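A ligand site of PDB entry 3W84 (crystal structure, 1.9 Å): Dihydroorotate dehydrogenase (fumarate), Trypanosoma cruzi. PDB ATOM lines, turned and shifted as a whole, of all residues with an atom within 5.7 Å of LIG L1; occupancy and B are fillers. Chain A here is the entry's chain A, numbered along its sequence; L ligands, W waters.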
ATOM      1  N   LYS A  44       1.575   4.475  -7.308  1.00  0.00           N
ATOM      2  CA  LYS A  44       2.089   4.582  -5.968  1.00  0.00           C
ATOM      3  C   LYS A  44       2.089   6.016  -5.524  1.00  0.00           C
ATOM      4  O   LYS A  44       2.529   6.889  -6.264  1.00  0.00           O
ATOM      5  CB  LYS A  44       3.493   4.064  -5.894  1.00  0.00           C
ATOM      6  CG  LYS A  44       4.244   4.380  -4.623  1.00  0.00           C
ATOM      7  CD  LYS A  44       3.714   3.755  -3.375  1.00  0.00           C
ATOM      8  CE  LYS A  44       4.436   4.321  -2.144  1.00  0.00           C
ATOM      9  NZ  LYS A  44       3.944   3.662  -0.890  1.00  0.00           N
ATOM     10  N   SER A  45       1.648   6.220  -4.284  1.00  0.00           N
ATOM     11  CA  SER A  45       1.659   7.564  -3.701  1.00  0.00           C
ATOM     12  C   SER A  45       3.068   8.166  -3.853  1.00  0.00           C
ATOM     13  O   SER A  45       4.024   7.562  -3.491  1.00  0.00           O
ATOM     14  CB  SER A  45       1.263   7.601  -2.234  1.00  0.00           C
ATOM     15  OG  SER A  45      -0.113   7.313  -2.018  1.00  0.00           O
ATOM     16  N   ARG A  51      12.187   8.563  -3.324  1.00  0.00           N
ATOM     17  CA  ARG A  51      12.458   8.135  -1.972  1.00  0.00           C
ATOM     18  C   ARG A  51      12.785   6.674  -1.935  1.00  0.00           C
ATOM     19  O   ARG A  51      12.058   5.872  -2.529  1.00  0.00           O
ATOM     20  CB  ARG A  51      11.243   8.313  -1.049  1.00  0.00           C
ATOM     21  CG  ARG A  51      10.943   9.779  -0.689  1.00  0.00           C
ATOM     22  CD  ARG A  51       9.681   9.902   0.137  1.00  0.00           C
ATOM     23  NE  ARG A  51       9.745   9.152   1.400  1.00  0.00           N
ATOM     24  CZ  ARG A  51      10.221   9.624   2.545  1.00  0.00           C
ATOM     25  NH1 ARG A  51      10.656  10.877   2.617  1.00  0.00           N
ATOM     26  NH2 ARG A  51      10.228   8.875   3.619  1.00  0.00           N
ATOM     27  N   ASN A  54      11.929   3.289   4.036  1.00  0.00           N
ATOM     28  CA  ASN A  54      12.493   2.794   5.295  1.00  0.00           C
ATOM     29  C   ASN A  54      13.350   1.554   5.112  1.00  0.00           C
ATOM     30  O   ASN A  54      13.245   0.873   4.082  1.00  0.00           O
ATOM     31  CB  ASN A  54      11.374   2.482   6.295  1.00  0.00           C
ATOM     32  CG  ASN A  54      10.803   3.711   6.946  1.00  0.00           C
ATOM     33  OD1 ASN A  54      11.462   4.784   6.970  1.00  0.00           O
ATOM     34  ND2 ASN A  54       9.591   3.587   7.454  1.00  0.00           N
ATOM     35  N   ASN A  68       2.918  -2.936   7.760  1.00  0.00           N
ATOM     36  CA  ASN A  68       3.948  -2.238   6.989  1.00  0.00           C
ATOM     37  C   ASN A  68       4.343  -0.893   7.604  1.00  0.00           C
ATOM     38  O   ASN A  68       3.551  -0.177   8.220  1.00  0.00           O
ATOM     39  CB  ASN A  68       3.502  -2.079   5.502  1.00  0.00           C
ATOM     40  CG  ASN A  68       2.721  -0.816   5.250  1.00  0.00           C
ATOM     41  OD1 ASN A  68       3.299   0.302   5.197  1.00  0.00           O
ATOM     42  ND2 ASN A  68       1.405  -0.941   5.203  1.00  0.00           N
ATOM     43  N   SER A  69       5.624  -0.568   7.453  1.00  0.00           N
ATOM     44  CA  SER A  69       6.039   0.825   7.585  1.00  0.00           C
ATOM     45  C   SER A  69       7.040   1.097   6.479  1.00  0.00           C
ATOM     46  O   SER A  69       8.275   1.066   6.688  1.00  0.00           O
ATOM     47  CB  SER A  69       6.653   1.072   8.932  1.00  0.00           C
ATOM     48  OG  SER A  69       7.129   2.408   8.965  1.00  0.00           O
ATOM     49  N   MET A  70       6.501   1.258   5.261  1.00  0.00           N
ATOM     50  CA  MET A  70       7.351   1.223   4.044  1.00  0.00           C
ATOM     51  C   MET A  70       8.173   2.527   4.038  1.00  0.00           C
ATOM     52  O   MET A  70       9.317   2.596   3.512  1.00  0.00           O
ATOM     53  CB  MET A  70       6.496   1.225   2.797  1.00  0.00           C
ATOM     54  CG  MET A  70       5.528   0.091   2.646  1.00  0.00           C
ATOM     55  SD  MET A  70       6.461  -1.410   2.615  1.00  0.00           S
ATOM     56  CE  MET A  70       7.265  -1.235   1.049  1.00  0.00           C
ATOM     57  N   GLY A  71       7.556   3.559   4.541  1.00  0.00           N
ATOM     58  CA  GLY A  71       8.137   4.859   4.505  1.00  0.00           C
ATOM     59  C   GLY A  71       8.095   5.628   3.170  1.00  0.00           C
ATOM     60  O   GLY A  71       9.057   6.416   2.874  1.00  0.00           O
ATOM     61  N   LEU A  72       7.008   5.460   2.419  1.00  0.00           N
ATOM     62  CA  LEU A  72       6.763   6.141   1.127  1.00  0.00           C
ATOM     63  C   LEU A  72       7.920   6.072   0.114  1.00  0.00           C
ATOM     64  O   LEU A  72       8.374   7.089  -0.433  1.00  0.00           O
ATOM     65  CB  LEU A  72       6.452   7.627   1.339  1.00  0.00           C
ATOM     66  CG  LEU A  72       5.063   8.165   1.073  1.00  0.00           C
ATOM     67  CD1 LEU A  72       5.090   9.691   1.293  1.00  0.00           C
ATOM     68  CD2 LEU A  72       4.524   7.772  -0.281  1.00  0.00           C
ATOM     69  N   PRO A  73       8.401   4.865  -0.151  1.00  0.00           N
ATOM     70  CA  PRO A  73       9.347   4.709  -1.242  1.00  0.00           C
ATOM     71  C   PRO A  73       8.641   4.901  -2.592  1.00  0.00           C
ATOM     72  O   PRO A  73       7.558   4.295  -2.801  1.00  0.00           O
ATOM     73  CB  PRO A  73       9.777   3.252  -1.114  1.00  0.00           C
ATOM     74  CG  PRO A  73       8.543   2.565  -0.668  1.00  0.00           C
ATOM     75  CD  PRO A  73       7.842   3.583   0.276  1.00  0.00           C
ATOM     76  N   SER A 100       1.134  11.957  -2.223  1.00  0.00           N
ATOM     77  CA  SER A 100       1.230  11.946  -0.786  1.00  0.00           C
ATOM     78  C   SER A 100       2.308  12.816  -0.250  1.00  0.00           C
ATOM     79  O   SER A 100       3.259  12.342   0.435  1.00  0.00           O
ATOM     80  CB  SER A 100       1.411  10.506  -0.316  1.00  0.00           C
ATOM     81  OG  SER A 100       1.333  10.468   1.089  1.00  0.00           O
ATOM     82  N   LEU A 102       4.556  15.476   1.848  1.00  0.00           N
ATOM     83  CA  LEU A 102       4.919  15.501   3.277  1.00  0.00           C
ATOM     84  C   LEU A 102       4.655  16.850   3.985  1.00  0.00           C
ATOM     85  O   LEU A 102       4.885  16.979   5.198  1.00  0.00           O
ATOM     86  CB  LEU A 102       6.413  15.116   3.462  1.00  0.00           C
ATOM     87  CG  LEU A 102       6.838  13.723   2.896  1.00  0.00           C
ATOM     88  CD1 LEU A 102       8.156  13.242   3.494  1.00  0.00           C
ATOM     89  CD2 LEU A 102       5.783  12.666   3.123  1.00  0.00           C
ATOM     90  N   ASN A 128      -3.581  11.600  -0.748  1.00  0.00           N
ATOM     91  CA  ASN A 128      -3.462  10.835   0.486  1.00  0.00           C
ATOM     92  C   ASN A 128      -3.403  11.714   1.707  1.00  0.00           C
ATOM     93  O   ASN A 128      -2.408  12.401   1.933  1.00  0.00           O
ATOM     94  CB  ASN A 128      -2.253   9.916   0.532  1.00  0.00           C
ATOM     95  CG  ASN A 128      -2.265   9.008   1.738  1.00  0.00           C
ATOM     96  OD1 ASN A 128      -3.295   8.717   2.308  1.00  0.00           O
ATOM     97  ND2 ASN A 128      -1.132   8.500   2.071  1.00  0.00           N
ATOM     98  N   SER A 130      -3.999  10.281   4.824  1.00  0.00           N
ATOM     99  CA  SER A 130      -3.508   9.427   5.889  1.00  0.00           C
ATOM    100  C   SER A 130      -1.985   9.416   5.805  1.00  0.00           C
ATOM    101  O   SER A 130      -1.364   8.423   5.346  1.00  0.00           O
ATOM    102  CB  SER A 130      -4.036   7.987   5.714  1.00  0.00           C
ATOM    103  OG  SER A 130      -3.610   7.203   6.794  1.00  0.00           O
ATOM    104  N   CYS A 131      -1.372  10.522   6.243  1.00  0.00           N
ATOM    105  CA  CYS A 131      -0.015  10.849   5.888  1.00  0.00           C
ATOM    106  C   CYS A 131       0.593  11.734   6.989  1.00  0.00           C
ATOM    107  O   CYS A 131      -0.082  12.622   7.454  1.00  0.00           O
ATOM    108  CB  CYS A 131      -0.038  11.672   4.582  1.00  0.00           C
ATOM    109  SG  CYS A 131       1.631  12.088   3.977  1.00  0.00           S
ATOM    110  N   PRO A 132       1.889  11.519   7.333  1.00  0.00           N
ATOM    111  CA  PRO A 132       2.532  12.388   8.335  1.00  0.00           C
ATOM    112  C   PRO A 132       2.598  13.837   7.882  1.00  0.00           C
ATOM    113  O   PRO A 132       2.599  14.145   6.713  1.00  0.00           O
ATOM    114  CB  PRO A 132       3.952  11.798   8.483  1.00  0.00           C
ATOM    115  CG  PRO A 132       4.121  10.884   7.331  1.00  0.00           C
ATOM    116  CD  PRO A 132       2.746  10.391   6.967  1.00  0.00           C
ATOM    117  N   GLN A 139      -1.178  12.360  12.228  1.00  0.00           N
ATOM    118  CA  GLN A 139      -1.261  12.368  10.796  1.00  0.00           C
ATOM    119  C   GLN A 139      -2.306  13.382  10.308  1.00  0.00           C
ATOM    120  O   GLN A 139      -3.294  13.742  11.033  1.00  0.00           O
ATOM    121  CB  GLN A 139      -1.620  10.977  10.310  1.00  0.00           C
ATOM    122  CG  GLN A 139      -3.002  10.558  10.741  1.00  0.00           C
ATOM    123  CD  GLN A 139      -3.597   9.599   9.759  1.00  0.00           C
ATOM    124  OE1 GLN A 139      -4.220  10.025   8.756  1.00  0.00           O
ATOM    125  NE2 GLN A 139      -3.427   8.307  10.027  1.00  0.00           N
ATOM    126  N   ASN A 195      -7.442   3.765   4.526  1.00  0.00           N
ATOM    127  CA  ASN A 195      -5.970   3.526   4.637  1.00  0.00           C
ATOM    128  C   ASN A 195      -5.753   2.503   5.742  1.00  0.00           C
ATOM    129  O   ASN A 195      -6.727   2.068   6.416  1.00  0.00           O
ATOM    130  CB  ASN A 195      -5.107   4.813   4.879  1.00  0.00           C
ATOM    131  CG  ASN A 195      -3.741   4.693   4.222  1.00  0.00           C
ATOM    132  OD1 ASN A 195      -3.039   3.683   4.390  1.00  0.00           O
ATOM    133  ND2 ASN A 195      -3.426   5.626   3.352  1.00  0.00           N
ATOM    134  N   SER A 196      -4.527   2.048   5.947  1.00  0.00           N
ATOM    135  CA  SER A 196      -4.320   1.048   7.007  1.00  0.00           C
ATOM    136  C   SER A 196      -4.739   1.497   8.375  1.00  0.00           C
ATOM    137  O   SER A 196      -4.800   2.730   8.687  1.00  0.00           O
ATOM    138  CB  SER A 196      -2.872   0.582   7.041  1.00  0.00           C
ATOM    139  OG  SER A 196      -2.049   1.593   6.667  1.00  0.00           O
ATOM    140  N   LYS A 215      10.384   1.941  13.297  1.00  0.00           N
ATOM    141  CA  LYS A 215       9.435   2.229  14.358  1.00  0.00           C
ATOM    142  C   LYS A 215       9.287   1.154  15.464  1.00  0.00           C
ATOM    143  O   LYS A 215       8.218   0.964  16.013  1.00  0.00           O
ATOM    144  CB  LYS A 215       8.065   2.537  13.757  1.00  0.00           C
ATOM    145  CG  LYS A 215       8.028   3.806  12.947  1.00  0.00           C
ATOM    146  CD  LYS A 215       6.623   4.063  12.381  1.00  0.00           C
ATOM    147  CE  LYS A 215       5.559   4.182  13.468  1.00  0.00           C
ATOM    148  NZ  LYS A 215       4.365   4.828  12.862  1.00  0.00           N
ATOM    149  N   GLY A 220       1.288   0.048   9.998  1.00  0.00           N
ATOM    150  CA  GLY A 220      -0.074  -0.066   9.612  1.00  0.00           C
ATOM    151  C   GLY A 220      -0.561  -1.466   9.283  1.00  0.00           C
ATOM    152  O   GLY A 220       0.083  -2.265   8.608  1.00  0.00           O
HETATM  153  O1  LIG L   1       4.455   4.284   2.557  1.00  0.00           O
HETATM  154  C1  LIG L   1       3.871   3.953   3.607  1.00  0.00           C
HETATM  155  O2  LIG L   1       4.502   3.598   4.615  1.00  0.00           O
HETATM  156  C2  LIG L   1       2.452   3.955   3.676  1.00  0.00           C
HETATM  157  N1  LIG L   1       1.852   2.738   4.174  1.00  0.00           N
HETATM  158  C3  LIG L   1       0.479   2.638   4.307  1.00  0.00           C
HETATM  159  O3  LIG L   1      -0.093   1.643   4.788  1.00  0.00           O
HETATM  160  N2  LIG L   1      -0.242   3.772   3.991  1.00  0.00           N
HETATM  161  C4  LIG L   1       0.297   4.952   3.521  1.00  0.00           C
HETATM  162  O4  LIG L   1      -0.522   5.846   3.259  1.00  0.00           O
HETATM  163  C5  LIG L   1       1.690   5.079   3.364  1.00  0.00           C
HETATM  164  C6  LIG L   1       2.315   6.234   2.939  1.00  0.00           C
HETATM  165  C7  LIG L   1       2.050   7.445   3.924  1.00  0.00           C
HETATM  166  C8  LIG L   1       3.117   7.389   4.891  1.00  0.00           C
HETATM  167  C9  LIG L   1       4.352   8.002   4.639  1.00  0.00           C
HETATM  168  C10 LIG L   1       5.417   7.931   5.546  1.00  0.00           C
HETATM  169  C11 LIG L   1       6.613   8.565   5.260  1.00  0.00           C
HETATM  170  C12 LIG L   1       7.676   8.459   6.181  1.00  0.00           C
HETATM  171  C13 LIG L   1       7.553   7.736   7.365  1.00  0.00           C
HETATM  172  C14 LIG L   1       6.339   7.106   7.637  1.00  0.00           C
HETATM  173  C15 LIG L   1       5.289   7.210   6.722  1.00  0.00           C
HETATM  174  C16 LIG L   1       4.081   6.603   6.987  1.00  0.00           C
HETATM  175  C17 LIG L   1       3.002   6.680   6.099  1.00  0.00           C
HETATM  176  O5  LIG L   1       1.795   6.092   6.369  1.00  0.00           O
HETATM  177  C18 LIG L   1       1.579   5.872   7.772  1.00  0.00           C
HETATM  178  O6  LIG L   1       0.492   6.695   8.177  1.00  0.00           O
HETATM  179  C19 LIG L   1       0.814   7.886   8.871  1.00  0.00           C
HETATM  180  N1  LG2 L   2      -1.898   3.768   0.949  1.00  0.00           N
HETATM  181  C1  LG2 L   2      -1.676   4.922   0.342  1.00  0.00           C
HETATM  182  O1  LG2 L   2      -2.634   5.726   0.275  1.00  0.00           O
HETATM  183  N2  LG2 L   2      -0.478   5.232  -0.162  1.00  0.00           N
HETATM  184  C2  LG2 L   2       0.566   4.368  -0.185  1.00  0.00           C
HETATM  185  O2  LG2 L   2       1.670   4.655  -0.710  1.00  0.00           O
HETATM  186  C3  LG2 L   2       0.384   3.071   0.409  1.00  0.00           C
HETATM  187  N3  LG2 L   2       1.351   2.131   0.444  1.00  0.00           N
HETATM  188  C4  LG2 L   2       1.074   0.897   0.929  1.00  0.00           C
HETATM  189  C5  LG2 L   2       2.039  -0.080   0.874  1.00  0.00           C
HETATM  190  C6  LG2 L   2       1.812  -1.346   1.395  1.00  0.00           C
HETATM  191  C7  LG2 L   2       2.946  -2.342   1.351  1.00  0.00           C
HETATM  192  C8  LG2 L   2       0.480  -1.670   1.967  1.00  0.00           C
HETATM  193  C9  LG2 L   2       0.175  -3.040   2.538  1.00  0.00           C
HETATM  194  C10 LG2 L   2      -0.490  -0.718   2.004  1.00  0.00           C
HETATM  195  C11 LG2 L   2      -0.268   0.553   1.498  1.00  0.00           C
HETATM  196  N4  LG2 L   2      -1.244   1.548   1.529  1.00  0.00           N
HETATM  197  C12 LG2 L   2      -0.957   2.809   0.945  1.00  0.00           C
HETATM  198  C13 LG2 L   2      -2.581   1.379   2.067  1.00  0.00           C
HETATM  199  C14 LG2 L   2      -3.396   0.433   1.210  1.00  0.00           C
HETATM  200  O3  LG2 L   2      -3.566   1.224   0.040  1.00  0.00           O
HETATM  201  C15 LG2 L   2      -4.700   0.105   1.949  1.00  0.00           C
HETATM  202  O4  LG2 L   2      -5.385   1.318   2.250  1.00  0.00           O
HETATM  203  C16 LG2 L   2      -4.529  -0.739   3.239  1.00  0.00           C
HETATM  204  O5  LG2 L   2      -3.480  -1.727   3.020  1.00  0.00           O
HETATM  205  C17 LG2 L   2      -5.866  -1.452   3.486  1.00  0.00           C
HETATM  206  O6  LG2 L   2      -6.223  -2.324   2.389  1.00  0.00           O
HETATM  207  P1  LG2 L   2      -6.046  -3.947   2.503  1.00  0.00           P
HETATM  208  O7  LG2 L   2      -6.605  -4.419   1.214  1.00  0.00           O
HETATM  209  O8  LG2 L   2      -6.776  -4.354   3.732  1.00  0.00           O
HETATM  210  O9  LG2 L   2      -4.539  -4.132   2.603  1.00  0.00           O
HETATM  211  O   HOH W   1       1.979   6.107  11.317  1.00  0.00           O
HETATM  212  O   HOH W   2       3.032   2.744   7.146  1.00  0.00           O
HETATM  213  O   HOH W   3      -0.194   3.083   7.237  1.00  0.00           O
HETATM  214  O   HOH W   4      -1.337   5.829   6.302  1.00  0.00           O
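A nitrogen (N1) of LG2 L2 lies close to a nitrogen (N2) of LIG L1, at 3.5 Å.
O of Ser 130 lies close to O4 of LIG L1.
NH2 of Arg 51 touches C12 of LIG L1, at 3.6 Å.
Pro 132 touches LIG L1 (CD to C8, 3.7 Å).
Hydrophobic or aromatic side chains within 4 Å of LIG L1: Met 70, Leu 72 and Pro 132.
Of the 21 residues printed, 11 come within 4 Å of LIG L1.
The nearest printed residue that does not touch LIG L1 is Ser 69 (4.02 Å).
The side-chain hydroxyl (OG) of Ser 196 sits at hydrogen-bond distance from the side-chain amide oxygen (OD1) of Asn 195 (3.2 Å).
O of Leu 72 sits at hydrogen-bond distance from NE of Arg 51 (3.1 Å).
ND2 of Asn 195 sits at hydrogen-bond distance from OD1 of Asn 128, 3.3 Å away.
OD1 of Asn 128 is in hydrogen-bond range of N of Ser 130, 3.0 Å away.
OG of Ser 100 sits at hydrogen-bond distance from ND2 of Asn 128 (3.3 Å).
The backbone NH of Met 70 is in hydrogen-bond range of the side-chain amide oxygen of Asn 68, 3.3 Å away.
N of Gly 220 is in hydrogen-bond range of O of Asn 68, at 2.9 Å.
OG of Ser 130 lies within hydrogen-bond range of NE2 of Gln 139 (3.4 Å).
Water W4 lies within hydrogen-bond range of OG of Ser 130, O6 of LIG L1 and OD1 of Asn 195.
Water W3 lies within hydrogen-bond range of OG of Ser 196 (2.4 Å) and O3 of LIG L1 (2.8 Å).
Water W2 bridges O2 of LIG L1 and OD1 of Asn 68.
An oxygen (O3) of LIG L1 sits at hydrogen-bond distance from the side-chain hydroxyl (OG) of Ser 196.
An oxygen (O1) of LIG L1 sits at hydrogen-bond distance from the backbone NH of Leu 72, at 2.8 Å.
OD1 of Asn 195 lies within hydrogen-bond range of N2 of LIG L1, 2.8 Å away.
O4 of LIG L1 sits at hydrogen-bond distance from ND2 of Asn 128 (3.0 Å).
OD1 of Asn 68 is in hydrogen-bond range of N1 of LIG L1, at 3.0 Å.
An oxygen (O2) of LIG L1 lies within hydrogen-bond range of the backbone NH (N) of Gly 71 (3.1 Å).
The backbone NH (N) of Met 70 lies within hydrogen-bond range of an oxygen (O2) of LIG L1.
An oxygen (O1) of LIG L1 lies within salt-bridge range of the side-chain amino group of Lys 44 (3.5 Å).
The side-chain amide nitrogen of Asn 195 lies within hydrogen-bond range of an oxygen (O1) of LG2 L2.
An oxygen (O2) of LG2 L2 sits at hydrogen-bond distance from the side-chain amino group (NZ) of Lys 44.
OG of Ser 45 sits at hydrogen-bond distance from N2 of LG2 L2 (2.8 Å).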
